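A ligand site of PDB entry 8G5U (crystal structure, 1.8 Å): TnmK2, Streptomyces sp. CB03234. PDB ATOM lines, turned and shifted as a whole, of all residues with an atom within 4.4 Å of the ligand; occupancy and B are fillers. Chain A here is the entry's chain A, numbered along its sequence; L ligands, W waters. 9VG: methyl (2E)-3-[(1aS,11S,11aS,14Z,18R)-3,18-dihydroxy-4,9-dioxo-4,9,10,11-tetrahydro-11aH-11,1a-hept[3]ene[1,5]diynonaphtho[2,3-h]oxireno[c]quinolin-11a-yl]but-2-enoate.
The side-chain carboxylate (OD1) of Asp 82 sits at hydrogen-bond distance from the side-chain hydroxyl (OG) of Ser 193, at 2.8 Å. NE2 of Gln 346 is in hydrogen-bond range of O of Leu 83 (2.9 Å). The backbone NH of Leu 228 sits close to the backbone carbonyl oxygen of Trp 223 (3.5 Å).
Water W2 bridges an oxygen (OAD) of the ligand and the side-chain amino group of Lys 338. Water W3 lies within hydrogen-bond range of OAD of the ligand (3.0 Å) and N of Phe 135 (3.4 Å). Water W1 lies within hydrogen-bond range of the side-chain hydroxyl (OG) of Ser 420 (2.7 Å), the side-chain carboxylate (OD2) of Asp 82 (2.9 Å), the side-chain amide oxygen (OD1) of Asn 301 (3.0 Å) and a nitrogen (NAT) of the ligand (3.0 Å). Water W5 lies within hydrogen-bond range of N of Val 134 (3.1 Å), OAF of the ligand (3.1 Å) and OE1 of Gln 346 (3.4 Å).
Merely in contact with the ligand: Val 134, Phe 135, Tyr 194, Leu 228, Phe 232, Leu 294, Gly 298, Phe 334, Lys 338, Met 381, Ser 420 and Thr 421. Hydrophobic or aromatic side chains that line the ligand: Leu 83, Val 134, Phe 135, Tyr 194, Leu 228, Phe 232, Leu 294, Phe 334 and Met 381. Within 4 Å of the ligand: Asp 82, Leu 83, Val 134, Phe 135, Ser 193, Tyr 194, Leu 228, Phe 232, Leu 294, Gly 298, Asn 301, Phe 334, Lys 338, Gln 346, Met 381, Ser 420 and Thr 421.
A nitrogen (NAT) of the ligand sits at hydrogen-bond distance from the side-chain carboxylate (OD2) of Asp 82 (3.4 Å). An oxygen (OAC) of the ligand lies within hydrogen-bond range of the side-chain hydroxyl (OG) of Ser 193 (3.1 Å). An oxygen (OAF) of the ligand is in hydrogen-bond range of the side-chain amide nitrogen (NE2) of Gln 346, 3.1 Å away. OAV of the ligand is in hydrogen-bond range of N of Leu 83 (3.3 Å). An oxygen (OAE) of the ligand is in hydrogen-bond range of the side-chain amide nitrogen (ND2) of Asn 301, 3.3 Å away.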
ATOM      1  N   ASP A  82      -5.483   3.062 -20.945  1.00  0.00           N
ATOM      2  CA  ASP A  82      -4.062   2.778 -20.958  1.00  0.00           C
ATOM      3  C   ASP A  82      -3.296   4.076 -21.138  1.00  0.00           C
ATOM      4  O   ASP A  82      -3.701   4.974 -21.887  1.00  0.00           O
ATOM      5  CB  ASP A  82      -3.753   1.754 -22.049  1.00  0.00           C
ATOM      6  CG  ASP A  82      -4.337   0.371 -21.725  1.00  0.00           C
ATOM      7  OD1 ASP A  82      -4.577   0.077 -20.528  1.00  0.00           O
ATOM      8  OD2 ASP A  82      -4.578  -0.416 -22.667  1.00  0.00           O
ATOM      9  N   LEU A  83      -2.216   4.225 -20.380  1.00  0.00           N
ATOM     10  CA  LEU A  83      -1.412   5.436 -20.455  1.00  0.00           C
ATOM     11  C   LEU A  83      -0.905   5.617 -21.878  1.00  0.00           C
ATOM     12  O   LEU A  83      -0.293   4.708 -22.452  1.00  0.00           O
ATOM     13  CB  LEU A  83      -0.252   5.346 -19.454  1.00  0.00           C
ATOM     14  CG  LEU A  83       0.778   6.476 -19.468  1.00  0.00           C
ATOM     15  CD1 LEU A  83       0.111   7.823 -19.183  1.00  0.00           C
ATOM     16  CD2 LEU A  83       1.881   6.207 -18.460  1.00  0.00           C
ATOM     17  N   PHE A 132       6.487   2.674 -30.461  1.00  0.00           N
ATOM     18  CA  PHE A 132       6.261   1.397 -29.797  1.00  0.00           C
ATOM     19  C   PHE A 132       7.374   1.050 -28.821  1.00  0.00           C
ATOM     20  O   PHE A 132       7.690  -0.125 -28.617  1.00  0.00           O
ATOM     21  CB  PHE A 132       6.099   0.290 -30.838  1.00  0.00           C
ATOM     22  CG  PHE A 132       4.806   0.376 -31.623  1.00  0.00           C
ATOM     23  CD1 PHE A 132       3.596   0.519 -30.980  1.00  0.00           C
ATOM     24  CD2 PHE A 132       4.822   0.320 -33.018  1.00  0.00           C
ATOM     25  CE1 PHE A 132       2.403   0.604 -31.697  1.00  0.00           C
ATOM     26  CE2 PHE A 132       3.638   0.404 -33.730  1.00  0.00           C
ATOM     27  CZ  PHE A 132       2.431   0.538 -33.076  1.00  0.00           C
ATOM     28  N   VAL A 134       7.483   0.925 -25.661  1.00  0.00           N
ATOM     29  CA  VAL A 134       7.094   0.124 -24.501  1.00  0.00           C
ATOM     30  C   VAL A 134       7.227  -1.360 -24.801  1.00  0.00           C
ATOM     31  O   VAL A 134       7.872  -2.097 -24.047  1.00  0.00           O
ATOM     32  CB  VAL A 134       5.659   0.487 -24.053  1.00  0.00           C
ATOM     33  CG1 VAL A 134       5.139  -0.535 -23.036  1.00  0.00           C
ATOM     34  CG2 VAL A 134       5.618   1.885 -23.440  1.00  0.00           C
ATOM     35  N   PHE A 135       6.612  -1.823 -25.889  1.00  0.00           N
ATOM     36  CA  PHE A 135       6.609  -3.238 -26.223  1.00  0.00           C
ATOM     37  C   PHE A 135       7.680  -3.607 -27.252  1.00  0.00           C
ATOM     38  O   PHE A 135       7.645  -4.712 -27.794  1.00  0.00           O
ATOM     39  CB  PHE A 135       5.221  -3.670 -26.729  1.00  0.00           C
ATOM     40  CG  PHE A 135       4.242  -3.957 -25.622  1.00  0.00           C
ATOM     41  CD1 PHE A 135       4.154  -5.220 -25.070  1.00  0.00           C
ATOM     42  CD2 PHE A 135       3.435  -2.949 -25.114  1.00  0.00           C
ATOM     43  CE1 PHE A 135       3.275  -5.475 -24.034  1.00  0.00           C
ATOM     44  CE2 PHE A 135       2.549  -3.204 -24.083  1.00  0.00           C
ATOM     45  CZ  PHE A 135       2.469  -4.467 -23.543  1.00  0.00           C
ATOM     46  N   SER A 193      -7.289   1.387 -15.839  1.00  0.00           N
ATOM     47  CA  SER A 193      -5.856   1.216 -16.062  1.00  0.00           C
ATOM     48  C   SER A 193      -5.075   2.371 -15.427  1.00  0.00           C
ATOM     49  O   SER A 193      -5.119   2.543 -14.200  1.00  0.00           O
ATOM     50  CB  SER A 193      -5.605   1.090 -17.569  1.00  0.00           C
ATOM     51  OG  SER A 193      -4.247   0.767 -17.841  1.00  0.00           O
ATOM     52  N   TYR A 194      -4.353   3.174 -16.214  1.00  0.00           N
ATOM     53  CA  TYR A 194      -3.664   4.328 -15.624  1.00  0.00           C
ATOM     54  C   TYR A 194      -4.641   5.236 -14.884  1.00  0.00           C
ATOM     55  O   TYR A 194      -4.309   5.808 -13.837  1.00  0.00           O
ATOM     56  CB  TYR A 194      -2.908   5.114 -16.701  1.00  0.00           C
ATOM     57  CG  TYR A 194      -2.232   6.371 -16.159  1.00  0.00           C
ATOM     58  CD1 TYR A 194      -1.275   6.307 -15.157  1.00  0.00           C
ATOM     59  CD2 TYR A 194      -2.581   7.617 -16.642  1.00  0.00           C
ATOM     60  CE1 TYR A 194      -0.676   7.454 -14.651  1.00  0.00           C
ATOM     61  CE2 TYR A 194      -1.985   8.772 -16.147  1.00  0.00           C
ATOM     62  CZ  TYR A 194      -1.046   8.696 -15.157  1.00  0.00           C
ATOM     63  OH  TYR A 194      -0.487   9.863 -14.678  1.00  0.00           O
ATOM     64  N   CYS A 219      -4.351  -0.831 -11.799  1.00  0.00           N
ATOM     65  CA  CYS A 219      -2.913  -0.729 -11.659  1.00  0.00           C
ATOM     66  C   CYS A 219      -2.496  -1.087 -10.227  1.00  0.00           C
ATOM     67  O   CYS A 219      -3.101  -0.641  -9.259  1.00  0.00           O
ATOM     68  CB  CYS A 219      -2.513   0.707 -12.022  1.00  0.00           C
ATOM     69  SG  CYS A 219      -0.796   1.186 -11.870  1.00  0.00           S
ATOM     70  N   TRP A 223       3.633  -0.855  -8.457  1.00  0.00           N
ATOM     71  CA  TRP A 223       4.247  -0.927  -9.770  1.00  0.00           C
ATOM     72  C   TRP A 223       5.111   0.279 -10.135  1.00  0.00           C
ATOM     73  O   TRP A 223       5.897   0.172 -11.078  1.00  0.00           O
ATOM     74  CB  TRP A 223       3.161  -1.051 -10.839  1.00  0.00           C
ATOM     75  CG  TRP A 223       2.697  -2.443 -11.131  1.00  0.00           C
ATOM     76  CD1 TRP A 223       3.163  -3.620 -10.608  1.00  0.00           C
ATOM     77  CD2 TRP A 223       1.661  -2.793 -12.054  1.00  0.00           C
ATOM     78  NE1 TRP A 223       2.483  -4.683 -11.155  1.00  0.00           N
ATOM     79  CE2 TRP A 223       1.550  -4.198 -12.044  1.00  0.00           C
ATOM     80  CE3 TRP A 223       0.824  -2.058 -12.884  1.00  0.00           C
ATOM     81  CZ2 TRP A 223       0.632  -4.881 -12.837  1.00  0.00           C
ATOM     82  CZ3 TRP A 223      -0.085  -2.727 -13.671  1.00  0.00           C
ATOM     83  CH2 TRP A 223      -0.180  -4.114 -13.644  1.00  0.00           C
ATOM     84  N   TRP A 225       7.496   2.686 -11.375  1.00  0.00           N
ATOM     85  CA  TRP A 225       6.782   2.363 -12.611  1.00  0.00           C
ATOM     86  C   TRP A 225       7.380   1.169 -13.375  1.00  0.00           C
ATOM     87  O   TRP A 225       6.790   0.721 -14.352  1.00  0.00           O
ATOM     88  CB  TRP A 225       6.728   3.571 -13.560  1.00  0.00           C
ATOM     89  CG  TRP A 225       5.563   4.476 -13.283  1.00  0.00           C
ATOM     90  CD1 TRP A 225       5.585   5.822 -13.102  1.00  0.00           C
ATOM     91  CD2 TRP A 225       4.194   4.071 -13.142  1.00  0.00           C
ATOM     92  NE1 TRP A 225       4.311   6.294 -12.868  1.00  0.00           N
ATOM     93  CE2 TRP A 225       3.437   5.230 -12.872  1.00  0.00           C
ATOM     94  CE3 TRP A 225       3.527   2.839 -13.204  1.00  0.00           C
ATOM     95  CZ2 TRP A 225       2.064   5.201 -12.676  1.00  0.00           C
ATOM     96  CZ3 TRP A 225       2.162   2.809 -13.002  1.00  0.00           C
ATOM     97  CH2 TRP A 225       1.439   3.979 -12.745  1.00  0.00           C
ATOM     98  N   LEU A 228       5.219  -2.249 -13.512  1.00  0.00           N
ATOM     99  CA  LEU A 228       4.231  -2.350 -14.577  1.00  0.00           C
ATOM    100  C   LEU A 228       4.778  -3.175 -15.742  1.00  0.00           C
ATOM    101  O   LEU A 228       4.037  -3.950 -16.370  1.00  0.00           O
ATOM    102  CB  LEU A 228       3.867  -0.939 -15.054  1.00  0.00           C
ATOM    103  CG  LEU A 228       3.158  -0.725 -16.392  1.00  0.00           C
ATOM    104  CD1 LEU A 228       1.738  -1.270 -16.352  1.00  0.00           C
ATOM    105  CD2 LEU A 228       3.161   0.763 -16.749  1.00  0.00           C
ATOM    106  N   PHE A 232       4.527  -7.894 -16.363  1.00  0.00           N
ATOM    107  CA  PHE A 232       3.689  -8.248 -17.510  1.00  0.00           C
ATOM    108  C   PHE A 232       3.975  -9.643 -18.071  1.00  0.00           C
ATOM    109  O   PHE A 232       3.012 -10.372 -18.356  1.00  0.00           O
ATOM    110  CB  PHE A 232       3.836  -7.196 -18.615  1.00  0.00           C
ATOM    111  CG  PHE A 232       2.918  -7.431 -19.778  1.00  0.00           C
ATOM    112  CD1 PHE A 232       3.262  -8.334 -20.785  1.00  0.00           C
ATOM    113  CD2 PHE A 232       1.701  -6.793 -19.863  1.00  0.00           C
ATOM    114  CE1 PHE A 232       2.421  -8.569 -21.847  1.00  0.00           C
ATOM    115  CE2 PHE A 232       0.849  -7.018 -20.924  1.00  0.00           C
ATOM    116  CZ  PHE A 232       1.214  -7.917 -21.925  1.00  0.00           C
ATOM    117  N   LEU A 294       3.110  -7.469 -30.667  1.00  0.00           N
ATOM    118  CA  LEU A 294       2.200  -6.432 -30.196  1.00  0.00           C
ATOM    119  C   LEU A 294       0.804  -6.573 -30.807  1.00  0.00           C
ATOM    120  O   LEU A 294      -0.186  -6.224 -30.156  1.00  0.00           O
ATOM    121  CB  LEU A 294       2.759  -5.045 -30.518  1.00  0.00           C
ATOM    122  CG  LEU A 294       2.001  -3.839 -29.946  1.00  0.00           C
ATOM    123  CD1 LEU A 294       1.810  -3.950 -28.437  1.00  0.00           C
ATOM    124  CD2 LEU A 294       2.739  -2.568 -30.289  1.00  0.00           C
ATOM    125  N   GLY A 298      -2.383  -6.789 -28.398  1.00  0.00           N
ATOM    126  CA  GLY A 298      -3.559  -5.980 -28.650  1.00  0.00           C
ATOM    127  C   GLY A 298      -4.822  -6.812 -28.729  1.00  0.00           C
ATOM    128  O   GLY A 298      -5.870  -6.416 -28.196  1.00  0.00           O
ATOM    129  N   ASN A 301      -6.182  -8.128 -25.222  1.00  0.00           N
ATOM    130  CA  ASN A 301      -6.842  -7.203 -24.299  1.00  0.00           C
ATOM    131  C   ASN A 301      -8.325  -7.537 -24.134  1.00  0.00           C
ATOM    132  O   ASN A 301      -8.958  -7.007 -23.215  1.00  0.00           O
ATOM    133  CB  ASN A 301      -6.675  -5.761 -24.765  1.00  0.00           C
ATOM    134  CG  ASN A 301      -5.364  -5.126 -24.279  1.00  0.00           C
ATOM    135  OD1 ASN A 301      -4.876  -5.404 -23.186  1.00  0.00           O
ATOM    136  ND2 ASN A 301      -4.792  -4.260 -25.118  1.00  0.00           N
ATOM    137  N   MET A 333      -6.823  -0.658 -35.107  1.00  0.00           N
ATOM    138  CA  MET A 333      -5.873  -0.703 -34.000  1.00  0.00           C
ATOM    139  C   MET A 333      -4.463  -0.329 -34.444  1.00  0.00           C
ATOM    140  O   MET A 333      -3.761   0.414 -33.748  1.00  0.00           O
ATOM    141  CB  MET A 333      -5.878  -2.107 -33.386  1.00  0.00           C
ATOM    142  CG  MET A 333      -5.051  -2.255 -32.118  1.00  0.00           C
ATOM    143  SD  MET A 333      -5.325  -3.837 -31.307  1.00  0.00           S
ATOM    144  CE  MET A 333      -7.027  -3.657 -30.754  1.00  0.00           C
ATOM    145  N   PHE A 334      -4.035  -0.831 -35.595  1.00  0.00           N
ATOM    146  CA  PHE A 334      -2.736  -0.468 -36.129  1.00  0.00           C
ATOM    147  C   PHE A 334      -2.967   0.422 -37.339  1.00  0.00           C
ATOM    148  O   PHE A 334      -3.330   1.590 -37.149  1.00  0.00           O
ATOM    149  CB  PHE A 334      -1.931  -1.742 -36.369  1.00  0.00           C
ATOM    150  CG  PHE A 334      -1.672  -2.496 -35.080  1.00  0.00           C
ATOM    151  CD1 PHE A 334      -0.609  -2.140 -34.251  1.00  0.00           C
ATOM    152  CD2 PHE A 334      -2.540  -3.489 -34.643  1.00  0.00           C
ATOM    153  CE1 PHE A 334      -0.395  -2.785 -33.048  1.00  0.00           C
ATOM    154  CE2 PHE A 334      -2.323  -4.142 -33.430  1.00  0.00           C
ATOM    155  CZ  PHE A 334      -1.248  -3.779 -32.635  1.00  0.00           C
ATOM    156  N   LYS A 338       0.958   4.994 -34.125  1.00  0.00           N
ATOM    157  CA  LYS A 338       0.527   5.326 -32.773  1.00  0.00           C
ATOM    158  C   LYS A 338       0.579   6.840 -32.580  1.00  0.00           C
ATOM    159  O   LYS A 338       1.533   7.500 -32.986  1.00  0.00           O
ATOM    160  CB  LYS A 338       1.439   4.619 -31.758  1.00  0.00           C
ATOM    161  CG  LYS A 338       0.956   4.619 -30.295  1.00  0.00           C
ATOM    162  CD  LYS A 338       2.075   4.165 -29.352  1.00  0.00           C
ATOM    163  CE  LYS A 338       1.610   3.921 -27.916  1.00  0.00           C
ATOM    164  NZ  LYS A 338       0.468   4.775 -27.486  1.00  0.00           N
ATOM    165  N   GLN A 346       3.225   9.611 -22.267  1.00  0.00           N
ATOM    166  CA  GLN A 346       3.433   8.321 -21.602  1.00  0.00           C
ATOM    167  C   GLN A 346       4.874   8.168 -21.107  1.00  0.00           C
ATOM    168  O   GLN A 346       5.107   7.787 -19.966  1.00  0.00           O
ATOM    169  CB  GLN A 346       3.056   7.218 -22.592  1.00  0.00           C
ATOM    170  CG  GLN A 346       3.565   5.839 -22.343  1.00  0.00           C
ATOM    171  CD  GLN A 346       3.358   4.964 -23.571  1.00  0.00           C
ATOM    172  OE1 GLN A 346       4.128   5.024 -24.525  1.00  0.00           O
ATOM    173  NE2 GLN A 346       2.282   4.183 -23.572  1.00  0.00           N
ATOM    174  N   LEU A 350       5.867   8.241 -17.033  1.00  0.00           N
ATOM    175  CA  LEU A 350       6.511   7.062 -16.468  1.00  0.00           C
ATOM    176  C   LEU A 350       7.876   7.386 -15.879  1.00  0.00           C
ATOM    177  O   LEU A 350       8.278   6.781 -14.876  1.00  0.00           O
ATOM    178  CB  LEU A 350       6.616   5.978 -17.538  1.00  0.00           C
ATOM    179  CG  LEU A 350       5.297   5.306 -17.968  1.00  0.00           C
ATOM    180  CD1 LEU A 350       5.521   4.374 -19.129  1.00  0.00           C
ATOM    181  CD2 LEU A 350       4.671   4.543 -16.789  1.00  0.00           C
ATOM    182  N   MET A 381       9.722  -6.591 -22.229  1.00  0.00           N
ATOM    183  CA  MET A 381       9.267  -5.929 -21.020  1.00  0.00           C
ATOM    184  C   MET A 381      10.374  -5.729 -19.983  1.00  0.00           C
ATOM    185  O   MET A 381      10.381  -4.718 -19.277  1.00  0.00           O
ATOM    186  CB  MET A 381       8.139  -6.753 -20.373  1.00  0.00           C
ATOM    187  CG  MET A 381       6.809  -6.651 -21.081  1.00  0.00           C
ATOM    188  SD  MET A 381       5.974  -5.083 -20.766  1.00  0.00           S
ATOM    189  CE  MET A 381       6.210  -4.221 -22.318  1.00  0.00           C
ATOM    190  N   SER A 420      -2.997  -7.224 -18.833  1.00  0.00           N
ATOM    191  CA  SER A 420      -2.104  -6.108 -18.538  1.00  0.00           C
ATOM    192  C   SER A 420      -2.312  -5.521 -17.154  1.00  0.00           C
ATOM    193  O   SER A 420      -1.381  -4.946 -16.585  1.00  0.00           O
ATOM    194  CB  SER A 420      -2.278  -5.003 -19.586  1.00  0.00           C
ATOM    195  OG  SER A 420      -3.508  -4.328 -19.409  1.00  0.00           O
ATOM    196  N   THR A 421      -3.530  -5.616 -16.606  1.00  0.00           N
ATOM    197  CA  THR A 421      -3.793  -5.264 -15.211  1.00  0.00           C
ATOM    198  C   THR A 421      -4.367  -6.516 -14.582  1.00  0.00           C
ATOM    199  O   THR A 421      -5.555  -6.834 -14.783  1.00  0.00           O
ATOM    200  CB  THR A 421      -4.753  -4.081 -15.085  1.00  0.00           C
ATOM    201  OG1 THR A 421      -5.897  -4.298 -15.925  1.00  0.00           O
ATOM    202  CG2 THR A 421      -4.075  -2.779 -15.478  1.00  0.00           C
HETATM  203  CAA 9VG L   1       0.201   3.123 -16.541  1.00  0.00           C
HETATM  204  OAU 9VG L   1      -0.853   2.321 -16.000  1.00  0.00           O
HETATM  205  CAW 9VG L   1      -1.278   1.156 -16.644  1.00  0.00           C
HETATM  206  OAC 9VG L   1      -1.845   0.330 -15.965  1.00  0.00           O
HETATM  207  CAN 9VG L   1      -1.003   1.031 -18.059  1.00  0.00           C
HETATM  208  CAX 9VG L   1      -1.065  -0.122 -18.753  1.00  0.00           C
HETATM  209  CAB 9VG L   1      -1.441  -1.463 -18.133  1.00  0.00           C
HETATM  210  CBJ 9VG L   1      -0.764  -0.127 -20.217  1.00  0.00           C
HETATM  211  OAV 9VG L   1      -1.066   1.130 -20.823  1.00  0.00           O
HETATM  212  CBK 9VG L   1       0.252   0.703 -21.039  1.00  0.00           C
HETATM  213  CAZ 9VG L   1       0.452   0.390 -22.495  1.00  0.00           C
HETATM  214  CAS 9VG L   1       1.350   1.083 -23.244  1.00  0.00           C
HETATM  215  CAY 9VG L   1       1.339   0.945 -24.653  1.00  0.00           C
HETATM  216  OAF 9VG L   1       2.293   1.635 -25.306  1.00  0.00           O
HETATM  217  CBF 9VG L   1       0.449   0.068 -25.281  1.00  0.00           C
HETATM  218  CBB 9VG L   1       0.545  -0.068 -26.721  1.00  0.00           C
HETATM  219  OAD 9VG L   1       1.400   0.548 -27.351  1.00  0.00           O
HETATM  220  CBD 9VG L   1      -0.417  -0.956 -27.387  1.00  0.00           C
HETATM  221  CAQ 9VG L   1      -0.571  -0.862 -28.767  1.00  0.00           C
HETATM  222  CAO 9VG L   1      -1.517  -1.676 -29.385  1.00  0.00           C
HETATM  223  CAP 9VG L   1      -2.128  -2.691 -28.649  1.00  0.00           C
HETATM  224  CAR 9VG L   1      -2.103  -2.661 -27.267  1.00  0.00           C
HETATM  225  CBE 9VG L   1      -1.234  -1.789 -26.628  1.00  0.00           C
HETATM  226  CBC 9VG L   1      -1.287  -1.716 -25.156  1.00  0.00           C
HETATM  227  OAE 9VG L   1      -2.029  -2.475 -24.546  1.00  0.00           O
HETATM  228  CBG 9VG L   1      -0.418  -0.716 -24.506  1.00  0.00           C
HETATM  229  CBA 9VG L   1      -0.474  -0.511 -23.128  1.00  0.00           C
HETATM  230  NAT 9VG L   1      -1.357  -1.313 -22.371  1.00  0.00           N
HETATM  231  CBI 9VG L   1      -1.034  -1.502 -20.959  1.00  0.00           C
HETATM  232  CAK 9VG L   1       0.218  -2.235 -20.729  1.00  0.00           C
HETATM  233  CAI 9VG L   1       1.269  -2.728 -20.491  1.00  0.00           C
HETATM  234  CAM 9VG L   1       2.579  -3.215 -20.183  1.00  0.00           C
HETATM  235  CAL 9VG L   1       3.532  -2.248 -20.138  1.00  0.00           C
HETATM  236  CAH 9VG L   1       2.973  -0.947 -20.204  1.00  0.00           C
HETATM  237  CAJ 9VG L   1       2.378   0.073 -20.227  1.00  0.00           C
HETATM  238  CBH 9VG L   1       1.494   1.236 -20.220  1.00  0.00           C
HETATM  239  OAG 9VG L   1       2.025   2.411 -20.746  1.00  0.00           O
HETATM  240  O   HOH W   1      -3.739  -3.045 -21.743  1.00  0.00           O
HETATM  241  O   HOH W   2      -0.825   2.164 -28.246  1.00  0.00           O
HETATM  242  O   HOH W   3       4.337   0.024 -27.543  1.00  0.00           O
HETATM  243  O   HOH W   4      -2.329   2.063 -25.969  1.00  0.00           O
HETATM  244  O   HOH W   5       4.978   2.422 -26.618  1.00  0.00           O
